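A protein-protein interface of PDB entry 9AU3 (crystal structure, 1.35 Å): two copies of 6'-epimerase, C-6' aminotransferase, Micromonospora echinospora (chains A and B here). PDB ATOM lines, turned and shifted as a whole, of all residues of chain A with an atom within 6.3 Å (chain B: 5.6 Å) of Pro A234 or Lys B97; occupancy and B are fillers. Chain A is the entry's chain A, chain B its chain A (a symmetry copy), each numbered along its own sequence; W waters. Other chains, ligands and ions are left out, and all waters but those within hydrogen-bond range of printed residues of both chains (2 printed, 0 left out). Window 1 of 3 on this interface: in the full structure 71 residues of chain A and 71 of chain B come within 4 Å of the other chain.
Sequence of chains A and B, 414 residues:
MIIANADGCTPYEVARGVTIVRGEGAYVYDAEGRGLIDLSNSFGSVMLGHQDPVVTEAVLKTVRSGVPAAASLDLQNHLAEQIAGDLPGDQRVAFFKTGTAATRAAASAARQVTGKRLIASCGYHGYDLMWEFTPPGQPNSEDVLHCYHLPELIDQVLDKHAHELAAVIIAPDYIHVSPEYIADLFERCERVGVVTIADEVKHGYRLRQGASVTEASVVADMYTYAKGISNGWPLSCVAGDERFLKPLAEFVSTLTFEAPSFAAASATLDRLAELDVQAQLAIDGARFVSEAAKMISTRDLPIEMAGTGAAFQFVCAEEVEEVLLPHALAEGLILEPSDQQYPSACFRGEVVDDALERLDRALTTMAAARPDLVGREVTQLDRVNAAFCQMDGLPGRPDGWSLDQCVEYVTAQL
Lys A97 touches Pro B234, and with the chains exchanged Pro A234 touches Lys B97. Pro B234 touches its own counterpart, Pro A234. Pro A234 touches Leu B255, and with the chains exchanged Leu A255 touches Pro B234. Pro A234 touches Glu B258, and with the chains exchanged Glu A258 touches Pro B234. Of the 13 pairs that touch across the chains among the printed residues, 9 have their exchanged pair printed and touching as well.
The side-chain hydroxyl (OG) of Ser A230 sits at hydrogen-bond distance from the backbone carbonyl oxygen (O) of Trp A233, 2.6 Å away. The side-chain carboxylate of Glu A258 is in hydrogen-bond range of the side-chain hydroxyl of Ser A261 (2.7 Å). NZ of Lys B97 is in salt-bridge range of OE2 of Glu B258 (2.7 Å). The side-chain hydroxyl (OG1) of Thr B98 lies within hydrogen-bond range of the backbone NH (N) of Ala B101, at 3.1 Å. The side-chain hydroxyl (OG) of Ser B236 lies within hydrogen-bond range of the backbone carbonyl oxygen (O) of Thr B98 (2.7 Å). The side-chain hydroxyl (OG) of Ser B261 is in hydrogen-bond range of the side-chain carboxylate (OE2) of Glu B258, at 2.7 Å.
Water W2 bridges OH of Tyr A127 (2.8 Å) and O of Ala B101 (2.8 Å). Water W1 lies within hydrogen-bond range of the side-chain carboxylate (OE1) of Glu B258 (3.1 Å) and the backbone carbonyl oxygen (O) of Gly A232 (3.4 Å).
Phe A96 touches none of the printed residues of chain B. Of the printed residues of chain B, Pro A234 touches Lys B97, Pro B234, Leu B255 and Glu B258. Of the printed residues of chain B, Leu A255 touches Pro B234 (3.9 Å). Of the printed residues of chain A, Phe B96 touches Tyr A127 (3.5 Å). Lys B97 touches just these residues of chain A: Thr A98 and Pro A234. Thr B256 touches none of the printed residues of chain A. The nearest residue of chain A that does not touch Lys B97 is Lys A97 (4.2 Å).
Of the 13 printed residues of chain A, 8 touch a printed residue of chain B. Hydrophobic or aromatic side chains of chain A within 4 Å of the printed part of chain B: Tyr A127, Pro A234 and Leu A255. Of the 13 printed residues of chain B, 7 touch a printed residue of chain A. Hydrophobic or aromatic side chains of chain B within 4 Å of the printed part of chain A: Phe B96, Ala B101, Pro B234 and Leu B255. Along chain B the printed residues that touch a printed residue of chain A span positions 96 to 258.
Among the printed residues, merely in contact across the chains: Lys A97 with Thr B98 (3.7 Å), Lys A97 with Pro B234 (3.7 Å), Thr A98 with Lys B97 (3.7 Å), Tyr A127 with Phe B96 (3.5 Å), Tyr A127 with Ala B101 (3.8 Å), Gly A232 with Leu B255 (3.4 Å), Trp A233 with Leu B255 (3.4 Å), Pro A234 with Lys B97 (3.7 Å), Pro A234 with Pro B234 (3.8 Å), Pro A234 with Leu B255 (3.9 Å), Pro A234 with Glu B258 (3.5 Å), Leu A255 with Pro B234 (3.9 Å) and Glu A258 with Pro B234 (3.5 Å).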
ATOM      1  N   PHE A  96     -23.083  26.401  18.649  1.00  0.00           N
ATOM      2  CA  PHE A  96     -24.354  25.870  18.179  1.00  0.00           C
ATOM      3  C   PHE A  96     -24.176  24.379  17.922  1.00  0.00           C
ATOM      4  O   PHE A  96     -23.104  23.810  18.166  1.00  0.00           O
ATOM      5  CB  PHE A  96     -24.845  26.662  16.959  1.00  0.00           C
ATOM      6  CG  PHE A  96     -25.091  28.095  17.263  1.00  0.00           C
ATOM      7  CD1 PHE A  96     -26.307  28.500  17.765  1.00  0.00           C
ATOM      8  CD2 PHE A  96     -24.072  29.040  17.126  1.00  0.00           C
ATOM      9  CE1 PHE A  96     -26.538  29.825  18.098  1.00  0.00           C
ATOM     10  CE2 PHE A  96     -24.285  30.368  17.460  1.00  0.00           C
ATOM     11  CZ  PHE A  96     -25.526  30.761  17.961  1.00  0.00           C
ATOM     12  N   LYS A  97     -25.237  23.723  17.448  1.00  0.00           N
ATOM     13  CA  LYS A  97     -25.188  22.280  17.267  1.00  0.00           C
ATOM     14  C   LYS A  97     -25.125  21.836  15.810  1.00  0.00           C
ATOM     15  O   LYS A  97     -24.776  20.677  15.557  1.00  0.00           O
ATOM     16  CB  LYS A  97     -26.381  21.605  17.969  1.00  0.00           C
ATOM     17  CG  LYS A  97     -26.442  21.916  19.475  1.00  0.00           C
ATOM     18  CD  LYS A  97     -25.162  21.509  20.222  1.00  0.00           C
ATOM     19  CE  LYS A  97     -25.185  20.038  20.604  1.00  0.00           C
ATOM     20  NZ  LYS A  97     -23.816  19.512  20.939  1.00  0.00           N
ATOM     21  N   THR A  98     -25.453  22.710  14.860  1.00  0.00           N
ATOM     22  CA  THR A  98     -25.373  22.407  13.434  1.00  0.00           C
ATOM     23  C   THR A  98     -24.825  23.617  12.688  1.00  0.00           C
ATOM     24  O   THR A  98     -24.859  24.754  13.176  1.00  0.00           O
ATOM     25  CB  THR A  98     -26.753  22.097  12.823  1.00  0.00           C
ATOM     26  OG1 THR A  98     -27.571  23.271  12.879  1.00  0.00           O
ATOM     27  CG2 THR A  98     -27.441  20.930  13.529  1.00  0.00           C
ATOM     28  N   TYR A 127     -30.073  24.247   5.741  1.00  0.00           N
ATOM     29  CA  TYR A 127     -31.396  23.809   5.292  1.00  0.00           C
ATOM     30  C   TYR A 127     -32.498  24.828   5.571  1.00  0.00           C
ATOM     31  O   TYR A 127     -33.605  24.687   5.039  1.00  0.00           O
ATOM     32  CB  TYR A 127     -31.759  22.465   5.947  1.00  0.00           C
ATOM     33  CG  TYR A 127     -32.005  22.589   7.418  1.00  0.00           C
ATOM     34  CD1 TYR A 127     -33.213  23.094   7.899  1.00  0.00           C
ATOM     35  CD2 TYR A 127     -31.028  22.228   8.336  1.00  0.00           C
ATOM     36  CE1 TYR A 127     -33.431  23.245   9.254  1.00  0.00           C
ATOM     37  CE2 TYR A 127     -31.235  22.380   9.699  1.00  0.00           C
ATOM     38  CZ  TYR A 127     -32.437  22.877  10.149  1.00  0.00           C
ATOM     39  OH  TYR A 127     -32.649  23.032  11.499  1.00  0.00           O
ATOM     40  N   SER A 230     -15.120  18.636  14.825  1.00  0.00           N
ATOM     41  CA  SER A 230     -15.620  17.745  15.866  1.00  0.00           C
ATOM     42  C   SER A 230     -15.711  16.275  15.475  1.00  0.00           C
ATOM     43  O   SER A 230     -16.287  15.489  16.238  1.00  0.00           O
ATOM     44  CB  SER A 230     -16.973  18.239  16.365  1.00  0.00           C
ATOM     45  OG  SER A 230     -17.851  18.328  15.275  1.00  0.00           O
ATOM     46  N   GLY A 232     -17.460  14.356  13.560  1.00  0.00           N
ATOM     47  CA  GLY A 232     -18.752  13.697  13.493  1.00  0.00           C
ATOM     48  C   GLY A 232     -19.659  13.926  14.682  1.00  0.00           C
ATOM     49  O   GLY A 232     -20.759  13.358  14.718  1.00  0.00           O
ATOM     50  N   TRP A 233     -19.233  14.728  15.660  1.00  0.00           N
ATOM     51  CA  TRP A 233     -20.058  15.093  16.804  1.00  0.00           C
ATOM     52  C   TRP A 233     -20.742  16.431  16.534  1.00  0.00           C
ATOM     53  O   TRP A 233     -20.176  17.293  15.852  1.00  0.00           O
ATOM     54  CB  TRP A 233     -19.188  15.157  18.064  1.00  0.00           C
ATOM     55  CG  TRP A 233     -18.773  13.756  18.437  1.00  0.00           C
ATOM     56  CD1 TRP A 233     -17.758  13.017  17.883  1.00  0.00           C
ATOM     57  CD2 TRP A 233     -19.432  12.895  19.365  1.00  0.00           C
ATOM     58  NE1 TRP A 233     -17.732  11.758  18.442  1.00  0.00           N
ATOM     59  CE2 TRP A 233     -18.749  11.661  19.355  1.00  0.00           C
ATOM     60  CE3 TRP A 233     -20.523  13.055  20.223  1.00  0.00           C
ATOM     61  CZ2 TRP A 233     -19.131  10.592  20.164  1.00  0.00           C
ATOM     62  CZ3 TRP A 233     -20.901  11.996  21.025  1.00  0.00           C
ATOM     63  CH2 TRP A 233     -20.209  10.781  20.992  1.00  0.00           C
ATOM     64  N   PRO A 234     -21.982  16.622  17.007  1.00  0.00           N
ATOM     65  CA  PRO A 234     -22.766  17.794  16.586  1.00  0.00           C
ATOM     66  C   PRO A 234     -22.375  19.073  17.311  1.00  0.00           C
ATOM     67  O   PRO A 234     -22.955  19.415  18.348  1.00  0.00           O
ATOM     68  CB  PRO A 234     -24.206  17.381  16.920  1.00  0.00           C
ATOM     69  CG  PRO A 234     -24.049  16.427  18.066  1.00  0.00           C
ATOM     70  CD  PRO A 234     -22.767  15.677  17.821  1.00  0.00           C
ATOM     71  N   LEU A 235     -21.403  19.796  16.759  1.00  0.00           N
ATOM     72  CA  LEU A 235     -20.998  21.064  17.339  1.00  0.00           C
ATOM     73  C   LEU A 235     -20.592  21.999  16.212  1.00  0.00           C
ATOM     74  O   LEU A 235     -19.958  21.586  15.236  1.00  0.00           O
ATOM     75  CB  LEU A 235     -19.837  20.890  18.330  1.00  0.00           C
ATOM     76  CG  LEU A 235     -19.560  22.094  19.244  1.00  0.00           C
ATOM     77  CD1 LEU A 235     -20.722  22.365  20.188  1.00  0.00           C
ATOM     78  CD2 LEU A 235     -18.272  21.914  20.028  1.00  0.00           C
ATOM     79  N   SER A 236     -20.964  23.260  16.351  1.00  0.00           N
ATOM     80  CA  SER A 236     -20.632  24.286  15.374  1.00  0.00           C
ATOM     81  C   SER A 236     -20.394  25.589  16.120  1.00  0.00           C
ATOM     82  O   SER A 236     -20.616  25.681  17.332  1.00  0.00           O
ATOM     83  CB  SER A 236     -21.789  24.465  14.390  1.00  0.00           C
ATOM     84  OG  SER A 236     -22.914  24.967  15.090  1.00  0.00           O
ATOM     85  N   LEU A 255     -29.053  22.163  25.517  1.00  0.00           N
ATOM     86  CA  LEU A 255     -27.886  21.301  25.351  1.00  0.00           C
ATOM     87  C   LEU A 255     -26.790  21.934  24.498  1.00  0.00           C
ATOM     88  O   LEU A 255     -25.943  21.214  23.951  1.00  0.00           O
ATOM     89  CB  LEU A 255     -28.307  19.929  24.815  1.00  0.00           C
ATOM     90  CG  LEU A 255     -29.263  19.155  25.732  1.00  0.00           C
ATOM     91  CD1 LEU A 255     -29.666  17.848  25.091  1.00  0.00           C
ATOM     92  CD2 LEU A 255     -28.609  18.905  27.094  1.00  0.00           C
ATOM     93  N   GLU A 258     -23.751  20.520  26.171  1.00  0.00           N
ATOM     94  CA  GLU A 258     -23.541  19.116  26.513  1.00  0.00           C
ATOM     95  C   GLU A 258     -22.068  18.751  26.324  1.00  0.00           C
ATOM     96  O   GLU A 258     -21.398  19.195  25.378  1.00  0.00           O
ATOM     97  CB  GLU A 258     -24.471  18.163  25.735  1.00  0.00           C
ATOM     98  CG  GLU A 258     -24.455  18.291  24.209  1.00  0.00           C
ATOM     99  CD  GLU A 258     -23.517  17.300  23.516  1.00  0.00           C
ATOM    100  OE1 GLU A 258     -22.679  16.678  24.191  1.00  0.00           O
ATOM    101  OE2 GLU A 258     -23.609  17.158  22.279  1.00  0.00           O
ATOM    102  N   SER A 261     -19.795  16.428  23.136  1.00  0.00           N
ATOM    103  CA  SER A 261     -19.391  17.067  21.883  1.00  0.00           C
ATOM    104  C   SER A 261     -18.244  18.043  22.094  1.00  0.00           C
ATOM    105  O   SER A 261     -17.390  18.195  21.214  1.00  0.00           O
ATOM    106  CB  SER A 261     -20.573  17.761  21.215  1.00  0.00           C
ATOM    107  OG  SER A 261     -21.487  16.803  20.693  1.00  0.00           O
ATOM    108  N   PHE B  95     -36.454  14.973  12.273  1.00  0.00           N
ATOM    109  CA  PHE B  95     -35.525  15.091  13.393  1.00  0.00           C
ATOM    110  C   PHE B  95     -34.637  16.320  13.270  1.00  0.00           C
ATOM    111  O   PHE B  95     -34.216  16.688  12.169  1.00  0.00           O
ATOM    112  CB  PHE B  95     -34.659  13.836  13.534  1.00  0.00           C
ATOM    113  CG  PHE B  95     -35.433  12.637  13.988  1.00  0.00           C
ATOM    114  CD1 PHE B  95     -35.735  12.467  15.326  1.00  0.00           C
ATOM    115  CD2 PHE B  95     -35.883  11.691  13.081  1.00  0.00           C
ATOM    116  CE1 PHE B  95     -36.481  11.363  15.760  1.00  0.00           C
ATOM    117  CE2 PHE B  95     -36.621  10.582  13.506  1.00  0.00           C
ATOM    118  CZ  PHE B  95     -36.915  10.421  14.845  1.00  0.00           C
ATOM    119  N   PHE B  96     -34.341  16.928  14.421  1.00  0.00           N
ATOM    120  CA  PHE B  96     -33.466  18.085  14.546  1.00  0.00           C
ATOM    121  C   PHE B  96     -32.559  17.865  15.749  1.00  0.00           C
ATOM    122  O   PHE B  96     -32.604  16.814  16.402  1.00  0.00           O
ATOM    123  CB  PHE B  96     -34.295  19.376  14.612  1.00  0.00           C
ATOM    124  CG  PHE B  96     -35.103  19.606  13.388  1.00  0.00           C
ATOM    125  CD1 PHE B  96     -34.552  20.253  12.304  1.00  0.00           C
ATOM    126  CD2 PHE B  96     -36.400  19.101  13.281  1.00  0.00           C
ATOM    127  CE1 PHE B  96     -35.277  20.434  11.137  1.00  0.00           C
ATOM    128  CE2 PHE B  96     -37.136  19.269  12.119  1.00  0.00           C
ATOM    129  CZ  PHE B  96     -36.564  19.933  11.033  1.00  0.00           C
ATOM    130  N   LYS B  97     -31.705  18.847  16.043  1.00  0.00           N
ATOM    131  CA  LYS B  97     -30.735  18.680  17.115  1.00  0.00           C
ATOM    132  C   LYS B  97     -31.037  19.502  18.362  1.00  0.00           C
ATOM    133  O   LYS B  97     -30.466  19.209  19.419  1.00  0.00           O
ATOM    134  CB  LYS B  97     -29.314  18.995  16.612  1.00  0.00           C
ATOM    135  CG  LYS B  97     -28.894  18.118  15.419  1.00  0.00           C
ATOM    136  CD  LYS B  97     -28.963  16.614  15.730  1.00  0.00           C
ATOM    137  CE  LYS B  97     -27.702  16.132  16.429  1.00  0.00           C
ATOM    138  NZ  LYS B  97     -27.900  14.809  17.117  1.00  0.00           N
ATOM    139  N   THR B  98     -31.903  20.512  18.270  1.00  0.00           N
ATOM    140  CA  THR B  98     -32.305  21.325  19.414  1.00  0.00           C
ATOM    141  C   THR B  98     -33.799  21.609  19.333  1.00  0.00           C
ATOM    142  O   THR B  98     -34.425  21.512  18.269  1.00  0.00           O
ATOM    143  CB  THR B  98     -31.595  22.691  19.440  1.00  0.00           C
ATOM    144  OG1 THR B  98     -32.010  23.463  18.307  1.00  0.00           O
ATOM    145  CG2 THR B  98     -30.075  22.544  19.461  1.00  0.00           C
ATOM    146  N   GLY B  99     -34.374  21.976  20.478  1.00  0.00           N
ATOM    147  CA  GLY B  99     -35.776  22.377  20.491  1.00  0.00           C
ATOM    148  C   GLY B  99     -36.050  23.599  19.631  1.00  0.00           C
ATOM    149  O   GLY B  99     -37.084  23.669  18.956  1.00  0.00           O
ATOM    150  N   ALA B 101     -34.524  24.476  16.883  1.00  0.00           N
ATOM    151  CA  ALA B 101     -34.573  24.065  15.487  1.00  0.00           C
ATOM    152  C   ALA B 101     -35.913  23.410  15.179  1.00  0.00           C
ATOM    153  O   ALA B 101     -36.514  23.667  14.132  1.00  0.00           O
ATOM    154  CB  ALA B 101     -33.421  23.111  15.180  1.00  0.00           C
ATOM    155  N   PRO B 234     -28.342  15.503  22.265  1.00  0.00           N
ATOM    156  CA  PRO B 234     -28.970  16.557  21.454  1.00  0.00           C
ATOM    157  C   PRO B 234     -29.827  16.017  20.320  1.00  0.00           C
ATOM    158  O   PRO B 234     -29.348  15.833  19.195  1.00  0.00           O
ATOM    159  CB  PRO B 234     -27.763  17.339  20.915  1.00  0.00           C
ATOM    160  CG  PRO B 234     -26.667  16.316  20.863  1.00  0.00           C
ATOM    161  CD  PRO B 234     -26.890  15.396  22.034  1.00  0.00           C
ATOM    162  N   LEU B 235     -31.105  15.777  20.605  1.00  0.00           N
ATOM    163  CA  LEU B 235     -32.022  15.318  19.577  1.00  0.00           C
ATOM    164  C   LEU B 235     -33.395  15.906  19.860  1.00  0.00           C
ATOM    165  O   LEU B 235     -33.825  15.998  21.015  1.00  0.00           O
ATOM    166  CB  LEU B 235     -32.101  13.784  19.531  1.00  0.00           C
ATOM    167  CG  LEU B 235     -32.766  13.192  18.279  1.00  0.00           C
ATOM    168  CD1 LEU B 235     -31.964  13.488  17.020  1.00  0.00           C
ATOM    169  CD2 LEU B 235     -32.994  11.697  18.422  1.00  0.00           C
ATOM    170  N   SER B 236     -34.076  16.307  18.801  1.00  0.00           N
ATOM    171  CA  SER B 236     -35.414  16.870  18.899  1.00  0.00           C
ATOM    172  C   SER B 236     -36.201  16.433  17.674  1.00  0.00           C
ATOM    173  O   SER B 236     -35.655  15.828  16.746  1.00  0.00           O
ATOM    174  CB  SER B 236     -35.339  18.397  18.938  1.00  0.00           C
ATOM    175  OG  SER B 236     -34.828  18.864  17.703  1.00  0.00           O
ATOM    176  N   LEU B 255     -25.212  16.181  10.312  1.00  0.00           N
ATOM    177  CA  LEU B 255     -25.259  15.276  11.456  1.00  0.00           C
ATOM    178  C   LEU B 255     -26.660  15.123  12.044  1.00  0.00           C
ATOM    179  O   LEU B 255     -26.799  14.726  13.209  1.00  0.00           O
ATOM    180  CB  LEU B 255     -24.239  15.700  12.517  1.00  0.00           C
ATOM    181  CG  LEU B 255     -22.781  15.683  12.038  1.00  0.00           C
ATOM    182  CD1 LEU B 255     -21.861  16.174  13.131  1.00  0.00           C
ATOM    183  CD2 LEU B 255     -22.382  14.273  11.595  1.00  0.00           C
ATOM    184  N   THR B 256     -27.708  15.399  11.258  1.00  0.00           N
ATOM    185  CA  THR B 256     -29.062  15.119  11.738  1.00  0.00           C
ATOM    186  C   THR B 256     -29.165  13.693  12.252  1.00  0.00           C
ATOM    187  O   THR B 256     -29.816  13.430  13.275  1.00  0.00           O
ATOM    188  CB  THR B 256     -30.078  15.342  10.614  1.00  0.00           C
ATOM    189  OG1 THR B 256     -30.184  16.736  10.333  1.00  0.00           O
ATOM    190  CG2 THR B 256     -31.473  14.795  10.992  1.00  0.00           C
ATOM    191  N   GLU B 258     -26.534  11.542  13.136  1.00  0.00           N
ATOM    192  CA  GLU B 258     -25.463  10.924  13.912  1.00  0.00           C
ATOM    193  C   GLU B 258     -26.050   9.892  14.875  1.00  0.00           C
ATOM    194  O   GLU B 258     -27.123  10.083  15.469  1.00  0.00           O
ATOM    195  CB  GLU B 258     -24.582  11.956  14.647  1.00  0.00           C
ATOM    196  CG  GLU B 258     -25.313  12.955  15.549  1.00  0.00           C
ATOM    197  CD  GLU B 258     -25.358  12.538  17.021  1.00  0.00           C
ATOM    198  OE1 GLU B 258     -25.064  11.372  17.335  1.00  0.00           O
ATOM    199  OE2 GLU B 258     -25.713  13.384  17.868  1.00  0.00           O
ATOM    200  N   SER B 261     -26.839   9.874  19.359  1.00  0.00           N
ATOM    201  CA  SER B 261     -28.042  10.496  19.914  1.00  0.00           C
ATOM    202  C   SER B 261     -29.288   9.674  19.617  1.00  0.00           C
ATOM    203  O   SER B 261     -30.214   9.638  20.434  1.00  0.00           O
ATOM    204  CB  SER B 261     -28.206  11.924  19.407  1.00  0.00           C
ATOM    205  OG  SER B 261     -27.225  12.776  19.987  1.00  0.00           O
HETATM  206  O   HOH W   1     -21.984  11.873  17.580  1.00  0.00           O
HETATM  207  O   HOH W   2     -34.967  24.461  11.918  1.00  0.00           O
